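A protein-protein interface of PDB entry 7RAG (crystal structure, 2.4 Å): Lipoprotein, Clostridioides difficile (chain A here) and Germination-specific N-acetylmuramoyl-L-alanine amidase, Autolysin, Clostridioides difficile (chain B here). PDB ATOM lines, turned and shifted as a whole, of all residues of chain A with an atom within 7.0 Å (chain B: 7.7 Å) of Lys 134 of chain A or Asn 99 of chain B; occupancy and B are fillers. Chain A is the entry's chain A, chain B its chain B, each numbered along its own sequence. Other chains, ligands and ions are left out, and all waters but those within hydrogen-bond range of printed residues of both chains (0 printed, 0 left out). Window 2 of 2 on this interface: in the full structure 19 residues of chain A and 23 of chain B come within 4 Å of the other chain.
The side-chain amino group (NZ) of Lys 134 of chain A lies within hydrogen-bond range of the backbone carbonyl oxygen (O) of Asn 99 of chain B, at 3.3 Å.
The side-chain hydroxyl of Tyr 135 of chain A sits at hydrogen-bond distance from the backbone carbonyl oxygen of Ser 100 of chain B (2.6 Å).
OD1 of Asn 133 of chain A sits at hydrogen-bond distance from N of Tyr 135 of chain A (2.5 Å).
The backbone NH (N) of Phe 136 of chain A sits at hydrogen-bond distance from the side-chain amide oxygen (OD1) of Asn 133 of chain A.
The backbone carbonyl oxygen (O) of Lys 134 of chain A lies within hydrogen-bond range of the backbone NH (N) of Lys 158 of chain A, 2.8 Å away.
The backbone carbonyl oxygen (O) of Glu 95 of chain B sits at hydrogen-bond distance from the side-chain amide nitrogen (ND2) of Asn 99 of chain B, 2.6 Å away.
Ser 100 of chain B touches Lys 134 of chain A (O to NZ, 3.8 Å).
Asn 101 of chain B touches Lys 134 of chain A (OD1 to NZ, 3.7 Å).
Thr 18 of chain B touches Tyr 135 of chain A (OG1 to CD2, 3.3 Å).
CD2 of Leu 62 of chain B touches CD1 of Tyr 135 of chain A, 3.5 Å away.
Asn 101 of chain B touches Tyr 135 of chain A (O to CE2, 3.9 Å).
Thr 18 of chain B touches Phe 136 of chain A.
Lys 134 of chain A touches just these residues of chain B: Asn 99, Ser 100 and Asn 101.
Of the printed residues of chain B, Tyr 135 of chain A touches Thr 18, Leu 62, Ser 100 and Asn 101.
Printed residues of chain A within 4 Å of Thr 18 of chain B: Tyr 135 and Phe 136.
Of the printed residues of chain A, Leu 62 of chain B touches Tyr 135.
Asn 99 of chain B touches just one residue of chain A: Lys 134 (3.3 Å).
Of the printed residues of chain A, Asn 101 of chain B touches Lys 134 (3.7 Å) and Tyr 135 (3.9 Å).
The nearest residue of chain A that does not touch Asn 99 of chain B is Tyr 135 of chain A (5.1 Å).
Hydrophobic or aromatic side chains of chain B that line the printed part of chain A: Leu 62.
Hydrophobic or aromatic side chains of chain A within 4 Å of the printed part of chain B: Tyr 135 and Phe 136.
Among the printed residues, no Asp or Glu carboxylate lies within 4 Å of a Lys or Arg side-chain nitrogen of the other chain.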
ATOM      1  N   GLY A 131     -22.373  29.851 -35.537  1.00  0.00           N
ATOM      2  CA  GLY A 131     -22.992  28.699 -34.918  1.00  0.00           C
ATOM      3  C   GLY A 131     -24.048  29.056 -33.904  1.00  0.00           C
ATOM      4  O   GLY A 131     -24.787  28.163 -33.462  1.00  0.00           O
ATOM      5  N   ASP A 132     -24.143  30.334 -33.533  1.00  0.00           N
ATOM      6  CA  ASP A 132     -25.109  30.846 -32.558  1.00  0.00           C
ATOM      7  C   ASP A 132     -25.270  29.905 -31.363  1.00  0.00           C
ATOM      8  O   ASP A 132     -26.384  29.607 -30.923  1.00  0.00           O
ATOM      9  CB  ASP A 132     -26.459  31.129 -33.224  1.00  0.00           C
ATOM     10  N   ASN A 133     -24.128  29.419 -30.847  1.00  0.00           N
ATOM     11  CA  ASN A 133     -24.095  28.731 -29.556  1.00  0.00           C
ATOM     12  C   ASN A 133     -24.420  29.741 -28.461  1.00  0.00           C
ATOM     13  O   ASN A 133     -23.856  30.840 -28.427  1.00  0.00           O
ATOM     14  CB  ASN A 133     -22.717  28.085 -29.326  1.00  0.00           C
ATOM     15  CG  ASN A 133     -22.634  27.243 -28.037  1.00  0.00           C
ATOM     16  OD1 ASN A 133     -23.043  27.678 -26.965  1.00  0.00           O
ATOM     17  ND2 ASN A 133     -22.059  26.043 -28.141  1.00  0.00           N
ATOM     18  N   LYS A 134     -25.359  29.380 -27.587  1.00  0.00           N
ATOM     19  CA  LYS A 134     -25.712  30.242 -26.466  1.00  0.00           C
ATOM     20  C   LYS A 134     -24.478  30.635 -25.651  1.00  0.00           C
ATOM     21  O   LYS A 134     -24.381  31.771 -25.168  1.00  0.00           O
ATOM     22  CB  LYS A 134     -26.752  29.507 -25.606  1.00  0.00           C
ATOM     23  CG  LYS A 134     -27.018  30.028 -24.194  1.00  0.00           C
ATOM     24  CD  LYS A 134     -27.803  28.956 -23.435  1.00  0.00           C
ATOM     25  CE  LYS A 134     -28.500  29.469 -22.178  1.00  0.00           C
ATOM     26  NZ  LYS A 134     -29.492  28.446 -21.673  1.00  0.00           N
ATOM     27  N   TYR A 135     -23.506  29.732 -25.537  1.00  0.00           N
ATOM     28  CA  TYR A 135     -22.374  29.893 -24.640  1.00  0.00           C
ATOM     29  C   TYR A 135     -21.144  30.495 -25.296  1.00  0.00           C
ATOM     30  O   TYR A 135     -20.358  31.160 -24.611  1.00  0.00           O
ATOM     31  CB  TYR A 135     -22.004  28.539 -24.036  1.00  0.00           C
ATOM     32  CG  TYR A 135     -23.097  27.989 -23.168  1.00  0.00           C
ATOM     33  CD1 TYR A 135     -23.332  28.522 -21.904  1.00  0.00           C
ATOM     34  CD2 TYR A 135     -23.902  26.949 -23.608  1.00  0.00           C
ATOM     35  CE1 TYR A 135     -24.324  28.032 -21.106  1.00  0.00           C
ATOM     36  CE2 TYR A 135     -24.893  26.447 -22.817  1.00  0.00           C
ATOM     37  CZ  TYR A 135     -25.108  26.998 -21.562  1.00  0.00           C
ATOM     38  OH  TYR A 135     -26.107  26.519 -20.745  1.00  0.00           O
ATOM     39  N   PHE A 136     -20.935  30.247 -26.589  1.00  0.00           N
ATOM     40  CA  PHE A 136     -19.803  30.796 -27.332  1.00  0.00           C
ATOM     41  C   PHE A 136     -20.362  31.784 -28.348  1.00  0.00           C
ATOM     42  O   PHE A 136     -20.465  31.487 -29.536  1.00  0.00           O
ATOM     43  CB  PHE A 136     -18.986  29.664 -28.047  1.00  0.00           C
ATOM     44  CG  PHE A 136     -18.376  28.647 -27.116  1.00  0.00           C
ATOM     45  CD1 PHE A 136     -17.023  28.680 -26.822  1.00  0.00           C
ATOM     46  CD2 PHE A 136     -19.155  27.656 -26.541  1.00  0.00           C
ATOM     47  CE1 PHE A 136     -16.466  27.742 -25.983  1.00  0.00           C
ATOM     48  CE2 PHE A 136     -18.604  26.717 -25.704  1.00  0.00           C
ATOM     49  CZ  PHE A 136     -17.270  26.750 -25.429  1.00  0.00           C
ATOM     50  N   ASN A 137     -20.656  32.998 -27.893  1.00  0.00           N
ATOM     51  CA  ASN A 137     -21.372  33.939 -28.740  1.00  0.00           C
ATOM     52  C   ASN A 137     -20.455  34.949 -29.421  1.00  0.00           C
ATOM     53  O   ASN A 137     -20.518  35.131 -30.638  1.00  0.00           O
ATOM     54  CB  ASN A 137     -22.446  34.659 -27.933  1.00  0.00           C
ATOM     55  CG  ASN A 137     -23.547  35.177 -28.804  1.00  0.00           C
ATOM     56  OD1 ASN A 137     -24.216  34.403 -29.499  1.00  0.00           O
ATOM     57  ND2 ASN A 137     -23.741  36.490 -28.794  1.00  0.00           N
ATOM     58  N   LEU A 156     -17.800  35.497 -24.684  1.00  0.00           N
ATOM     59  CA  LEU A 156     -19.007  35.932 -23.998  1.00  0.00           C
ATOM     60  C   LEU A 156     -20.179  35.072 -24.449  1.00  0.00           C
ATOM     61  O   LEU A 156     -20.273  34.712 -25.629  1.00  0.00           O
ATOM     62  CB  LEU A 156     -19.303  37.405 -24.282  1.00  0.00           C
ATOM     63  CG  LEU A 156     -18.175  38.420 -24.083  1.00  0.00           C
ATOM     64  CD1 LEU A 156     -18.580  39.711 -24.754  1.00  0.00           C
ATOM     65  CD2 LEU A 156     -17.829  38.670 -22.611  1.00  0.00           C
ATOM     66  N   ASP A 157     -21.054  34.721 -23.504  1.00  0.00           N
ATOM     67  CA  ASP A 157     -22.266  34.013 -23.880  1.00  0.00           C
ATOM     68  C   ASP A 157     -23.256  34.997 -24.500  1.00  0.00           C
ATOM     69  O   ASP A 157     -22.954  36.174 -24.713  1.00  0.00           O
ATOM     70  CB  ASP A 157     -22.852  33.253 -22.686  1.00  0.00           C
ATOM     71  CG  ASP A 157     -23.288  34.150 -21.544  1.00  0.00           C
ATOM     72  OD1 ASP A 157     -23.541  35.351 -21.749  1.00  0.00           O
ATOM     73  OD2 ASP A 157     -23.400  33.626 -20.417  1.00  0.00           O
ATOM     74  N   LYS A 158     -24.458  34.519 -24.812  1.00  0.00           N
ATOM     75  CA  LYS A 158     -25.420  35.405 -25.458  1.00  0.00           C
ATOM     76  C   LYS A 158     -25.869  36.541 -24.546  1.00  0.00           C
ATOM     77  O   LYS A 158     -26.369  37.551 -25.049  1.00  0.00           O
ATOM     78  CB  LYS A 158     -26.634  34.611 -25.944  1.00  0.00           C
ATOM     79  CG  LYS A 158     -27.331  35.229 -27.144  1.00  0.00           C
ATOM     80  CD  LYS A 158     -28.558  34.421 -27.528  1.00  0.00           C
ATOM     81  CE  LYS A 158     -28.262  32.923 -27.467  1.00  0.00           C
ATOM     82  NZ  LYS A 158     -27.226  32.480 -28.466  1.00  0.00           N
ATOM     83  N   GLU A 159     -25.703  36.407 -23.228  1.00  0.00           N
ATOM     84  CA  GLU A 159     -26.038  37.465 -22.283  1.00  0.00           C
ATOM     85  C   GLU A 159     -24.858  38.379 -21.970  1.00  0.00           C
ATOM     86  O   GLU A 159     -24.955  39.195 -21.045  1.00  0.00           O
ATOM     87  CB  GLU A 159     -26.570  36.875 -20.973  1.00  0.00           C
ATOM     88  CG  GLU A 159     -27.259  35.539 -21.121  1.00  0.00           C
ATOM     89  CD  GLU A 159     -28.557  35.647 -21.871  1.00  0.00           C
ATOM     90  OE1 GLU A 159     -29.393  36.502 -21.498  1.00  0.00           O
ATOM     91  OE2 GLU A 159     -28.740  34.887 -22.844  1.00  0.00           O
ATOM     92  N   GLY A 160     -23.742  38.243 -22.691  1.00  0.00           N
ATOM     93  CA  GLY A 160     -22.592  39.093 -22.474  1.00  0.00           C
ATOM     94  C   GLY A 160     -21.678  38.675 -21.344  1.00  0.00           C
ATOM     95  O   GLY A 160     -20.700  39.385 -21.066  1.00  0.00           O
ATOM     96  N   ARG A 163     -17.554  33.600 -20.462  1.00  0.00           N
ATOM     97  CA  ARG A 163     -17.445  32.203 -20.079  1.00  0.00           C
ATOM     98  C   ARG A 163     -16.009  31.726 -20.062  1.00  0.00           C
ATOM     99  O   ARG A 163     -15.678  30.841 -19.270  1.00  0.00           O
ATOM    100  CB  ARG A 163     -18.259  31.324 -21.028  1.00  0.00           C
ATOM    101  CG  ARG A 163     -19.714  31.619 -20.994  1.00  0.00           C
ATOM    102  CD  ARG A 163     -20.145  31.686 -19.568  1.00  0.00           C
ATOM    103  NE  ARG A 163     -21.589  31.652 -19.473  1.00  0.00           N
ATOM    104  CZ  ARG A 163     -22.271  30.806 -18.721  1.00  0.00           C
ATOM    105  NH1 ARG A 163     -21.623  29.923 -17.973  1.00  0.00           N
ATOM    106  NH2 ARG A 163     -23.599  30.876 -18.717  1.00  0.00           N
ATOM    107  N   THR B  18     -20.564  22.214 -25.208  1.00  0.00           N
ATOM    108  CA  THR B  18     -20.994  22.355 -23.833  1.00  0.00           C
ATOM    109  C   THR B  18     -21.495  20.994 -23.374  1.00  0.00           C
ATOM    110  O   THR B  18     -22.340  20.385 -24.039  1.00  0.00           O
ATOM    111  CB  THR B  18     -22.067  23.439 -23.697  1.00  0.00           C
ATOM    112  OG1 THR B  18     -21.523  24.686 -24.156  1.00  0.00           O
ATOM    113  CG2 THR B  18     -22.490  23.620 -22.230  1.00  0.00           C
ATOM    114  N   ILE B  20     -22.681  18.366 -20.125  1.00  0.00           N
ATOM    115  CA  ILE B  20     -23.213  18.208 -18.777  1.00  0.00           C
ATOM    116  C   ILE B  20     -22.545  16.997 -18.154  1.00  0.00           C
ATOM    117  O   ILE B  20     -22.632  15.890 -18.703  1.00  0.00           O
ATOM    118  CB  ILE B  20     -24.741  18.038 -18.764  1.00  0.00           C
ATOM    119  CG1 ILE B  20     -25.428  19.230 -19.416  1.00  0.00           C
ATOM    120  CG2 ILE B  20     -25.228  17.932 -17.334  1.00  0.00           C
ATOM    121  CD1 ILE B  20     -26.801  18.863 -20.056  1.00  0.00           C
ATOM    122  N   LEU B  62     -17.034  23.779 -22.456  1.00  0.00           N
ATOM    123  CA  LEU B  62     -17.696  24.357 -21.296  1.00  0.00           C
ATOM    124  C   LEU B  62     -18.432  23.251 -20.572  1.00  0.00           C
ATOM    125  O   LEU B  62     -19.143  22.475 -21.211  1.00  0.00           O
ATOM    126  CB  LEU B  62     -18.679  25.443 -21.712  1.00  0.00           C
ATOM    127  CG  LEU B  62     -19.128  26.310 -20.556  1.00  0.00           C
ATOM    128  CD1 LEU B  62     -17.965  27.161 -20.028  1.00  0.00           C
ATOM    129  CD2 LEU B  62     -20.256  27.191 -21.005  1.00  0.00           C
ATOM    130  N   LYS B  91     -35.558  15.267 -10.477  1.00  0.00           N
ATOM    131  CA  LYS B  91     -36.268  16.265 -11.275  1.00  0.00           C
ATOM    132  C   LYS B  91     -35.396  17.493 -11.521  1.00  0.00           C
ATOM    133  O   LYS B  91     -35.395  18.053 -12.623  1.00  0.00           O
ATOM    134  CB  LYS B  91     -37.583  16.666 -10.595  1.00  0.00           C
ATOM    135  N   ASN B  92     -34.648  17.930 -10.507  1.00  0.00           N
ATOM    136  CA  ASN B  92     -33.837  19.129 -10.670  1.00  0.00           C
ATOM    137  C   ASN B  92     -32.688  18.907 -11.658  1.00  0.00           C
ATOM    138  O   ASN B  92     -32.419  19.767 -12.513  1.00  0.00           O
ATOM    139  CB  ASN B  92     -33.327  19.581  -9.309  1.00  0.00           C
ATOM    140  CG  ASN B  92     -34.428  20.255  -8.478  1.00  0.00           C
ATOM    141  OD1 ASN B  92     -35.174  21.088  -8.985  1.00  0.00           O
ATOM    142  ND2 ASN B  92     -34.537  19.879  -7.206  1.00  0.00           N
ATOM    143  N   ARG B  93     -32.008  17.753 -11.558  1.00  0.00           N
ATOM    144  CA  ARG B  93     -31.012  17.384 -12.563  1.00  0.00           C
ATOM    145  C   ARG B  93     -31.629  17.325 -13.961  1.00  0.00           C
ATOM    146  O   ARG B  93     -31.026  17.785 -14.944  1.00  0.00           O
ATOM    147  CB  ARG B  93     -30.389  16.050 -12.185  1.00  0.00           C
ATOM    148  CG  ARG B  93     -29.891  16.053 -10.770  1.00  0.00           C
ATOM    149  CD  ARG B  93     -28.945  14.917 -10.452  1.00  0.00           C
ATOM    150  NE  ARG B  93     -28.482  15.077  -9.079  1.00  0.00           N
ATOM    151  CZ  ARG B  93     -27.345  14.598  -8.574  1.00  0.00           C
ATOM    152  NH1 ARG B  93     -26.495  13.906  -9.326  1.00  0.00           N
ATOM    153  NH2 ARG B  93     -27.053  14.824  -7.301  1.00  0.00           N
ATOM    154  N   LYS B  94     -32.846  16.785 -14.072  1.00  0.00           N
ATOM    155  CA  LYS B  94     -33.497  16.750 -15.374  1.00  0.00           C
ATOM    156  C   LYS B  94     -33.711  18.153 -15.919  1.00  0.00           C
ATOM    157  O   LYS B  94     -33.567  18.380 -17.126  1.00  0.00           O
ATOM    158  CB  LYS B  94     -34.828  16.007 -15.295  1.00  0.00           C
ATOM    159  CG  LYS B  94     -35.336  15.553 -16.658  1.00  0.00           C
ATOM    160  CD  LYS B  94     -34.422  14.459 -17.202  1.00  0.00           C
ATOM    161  CE  LYS B  94     -34.794  14.058 -18.603  1.00  0.00           C
ATOM    162  NZ  LYS B  94     -33.987  12.903 -19.053  1.00  0.00           N
ATOM    163  N   GLU B  95     -34.084  19.105 -15.055  1.00  0.00           N
ATOM    164  CA  GLU B  95     -34.322  20.466 -15.539  1.00  0.00           C
ATOM    165  C   GLU B  95     -33.016  21.120 -15.981  1.00  0.00           C
ATOM    166  O   GLU B  95     -32.993  21.901 -16.944  1.00  0.00           O
ATOM    167  CB  GLU B  95     -35.017  21.311 -14.478  1.00  0.00           C
ATOM    168  N   ILE B  96     -31.923  20.816 -15.281  1.00  0.00           N
ATOM    169  CA  ILE B  96     -30.623  21.310 -15.721  1.00  0.00           C
ATOM    170  C   ILE B  96     -30.315  20.794 -17.118  1.00  0.00           C
ATOM    171  O   ILE B  96     -29.812  21.535 -17.967  1.00  0.00           O
ATOM    172  CB  ILE B  96     -29.534  20.928 -14.712  1.00  0.00           C
ATOM    173  CG1 ILE B  96     -29.763  21.691 -13.416  1.00  0.00           C
ATOM    174  CG2 ILE B  96     -28.143  21.204 -15.281  1.00  0.00           C
ATOM    175  CD1 ILE B  96     -28.845  21.282 -12.318  1.00  0.00           C
ATOM    176  N   ILE B  97     -30.648  19.528 -17.391  1.00  0.00           N
ATOM    177  CA  ILE B  97     -30.458  18.996 -18.741  1.00  0.00           C
ATOM    178  C   ILE B  97     -31.358  19.723 -19.728  1.00  0.00           C
ATOM    179  O   ILE B  97     -30.928  20.115 -20.818  1.00  0.00           O
ATOM    180  CB  ILE B  97     -30.712  17.476 -18.781  1.00  0.00           C
ATOM    181  CG1 ILE B  97     -29.760  16.728 -17.844  1.00  0.00           C
ATOM    182  CG2 ILE B  97     -30.522  16.933 -20.192  1.00  0.00           C
ATOM    183  CD1 ILE B  97     -30.029  15.240 -17.811  1.00  0.00           C
ATOM    184  N   SER B  98     -32.627  19.906 -19.363  1.00  0.00           N
ATOM    185  CA  SER B  98     -33.588  20.475 -20.305  1.00  0.00           C
ATOM    186  C   SER B  98     -33.252  21.913 -20.671  1.00  0.00           C
ATOM    187  O   SER B  98     -33.377  22.304 -21.833  1.00  0.00           O
ATOM    188  CB  SER B  98     -34.992  20.409 -19.724  1.00  0.00           C
ATOM    189  OG  SER B  98     -35.442  19.074 -19.718  1.00  0.00           O
ATOM    190  N   ASN B  99     -32.847  22.720 -19.699  1.00  0.00           N
ATOM    191  CA  ASN B  99     -32.738  24.155 -19.898  1.00  0.00           C
ATOM    192  C   ASN B  99     -31.336  24.611 -20.310  1.00  0.00           C
ATOM    193  O   ASN B  99     -31.116  25.815 -20.489  1.00  0.00           O
ATOM    194  CB  ASN B  99     -33.186  24.875 -18.624  1.00  0.00           C
ATOM    195  CG  ASN B  99     -34.583  24.440 -18.168  1.00  0.00           C
ATOM    196  OD1 ASN B  99     -35.583  24.602 -18.889  1.00  0.00           O
ATOM    197  ND2 ASN B  99     -34.651  23.876 -16.964  1.00  0.00           N
ATOM    198  N   SER B 100     -30.403  23.683 -20.514  1.00  0.00           N
ATOM    199  CA  SER B 100     -29.003  24.035 -20.687  1.00  0.00           C
ATOM    200  C   SER B 100     -28.601  24.382 -22.113  1.00  0.00           C
ATOM    201  O   SER B 100     -27.650  25.145 -22.286  1.00  0.00           O
ATOM    202  CB  SER B 100     -28.121  22.891 -20.210  1.00  0.00           C
ATOM    203  OG  SER B 100     -28.193  22.804 -18.806  1.00  0.00           O
ATOM    204  N   ASN B 101     -29.278  23.854 -23.133  1.00  0.00           N
ATOM    205  CA  ASN B 101     -28.776  23.925 -24.518  1.00  0.00           C
ATOM    206  C   ASN B 101     -27.366  23.352 -24.614  1.00  0.00           C
ATOM    207  O   ASN B 101     -26.487  23.897 -25.282  1.00  0.00           O
ATOM    208  CB  ASN B 101     -28.807  25.354 -25.078  1.00  0.00           C
ATOM    209  CG  ASN B 101     -30.199  25.825 -25.377  1.00  0.00           C
ATOM    210  OD1 ASN B 101     -30.656  26.835 -24.841  1.00  0.00           O
ATOM    211  ND2 ASN B 101     -30.900  25.083 -26.228  1.00  0.00           N
ATOM    212  N   ALA B 102     -27.137  22.265 -23.901  1.00  0.00           N
ATOM    213  CA  ALA B 102     -25.865  21.575 -23.977  1.00  0.00           C
ATOM    214  C   ALA B 102     -25.813  20.681 -25.221  1.00  0.00           C
ATOM    215  O   ALA B 102     -26.819  20.429 -25.898  1.00  0.00           O
ATOM    216  CB  ALA B 102     -25.641  20.754 -22.713  1.00  0.00           C
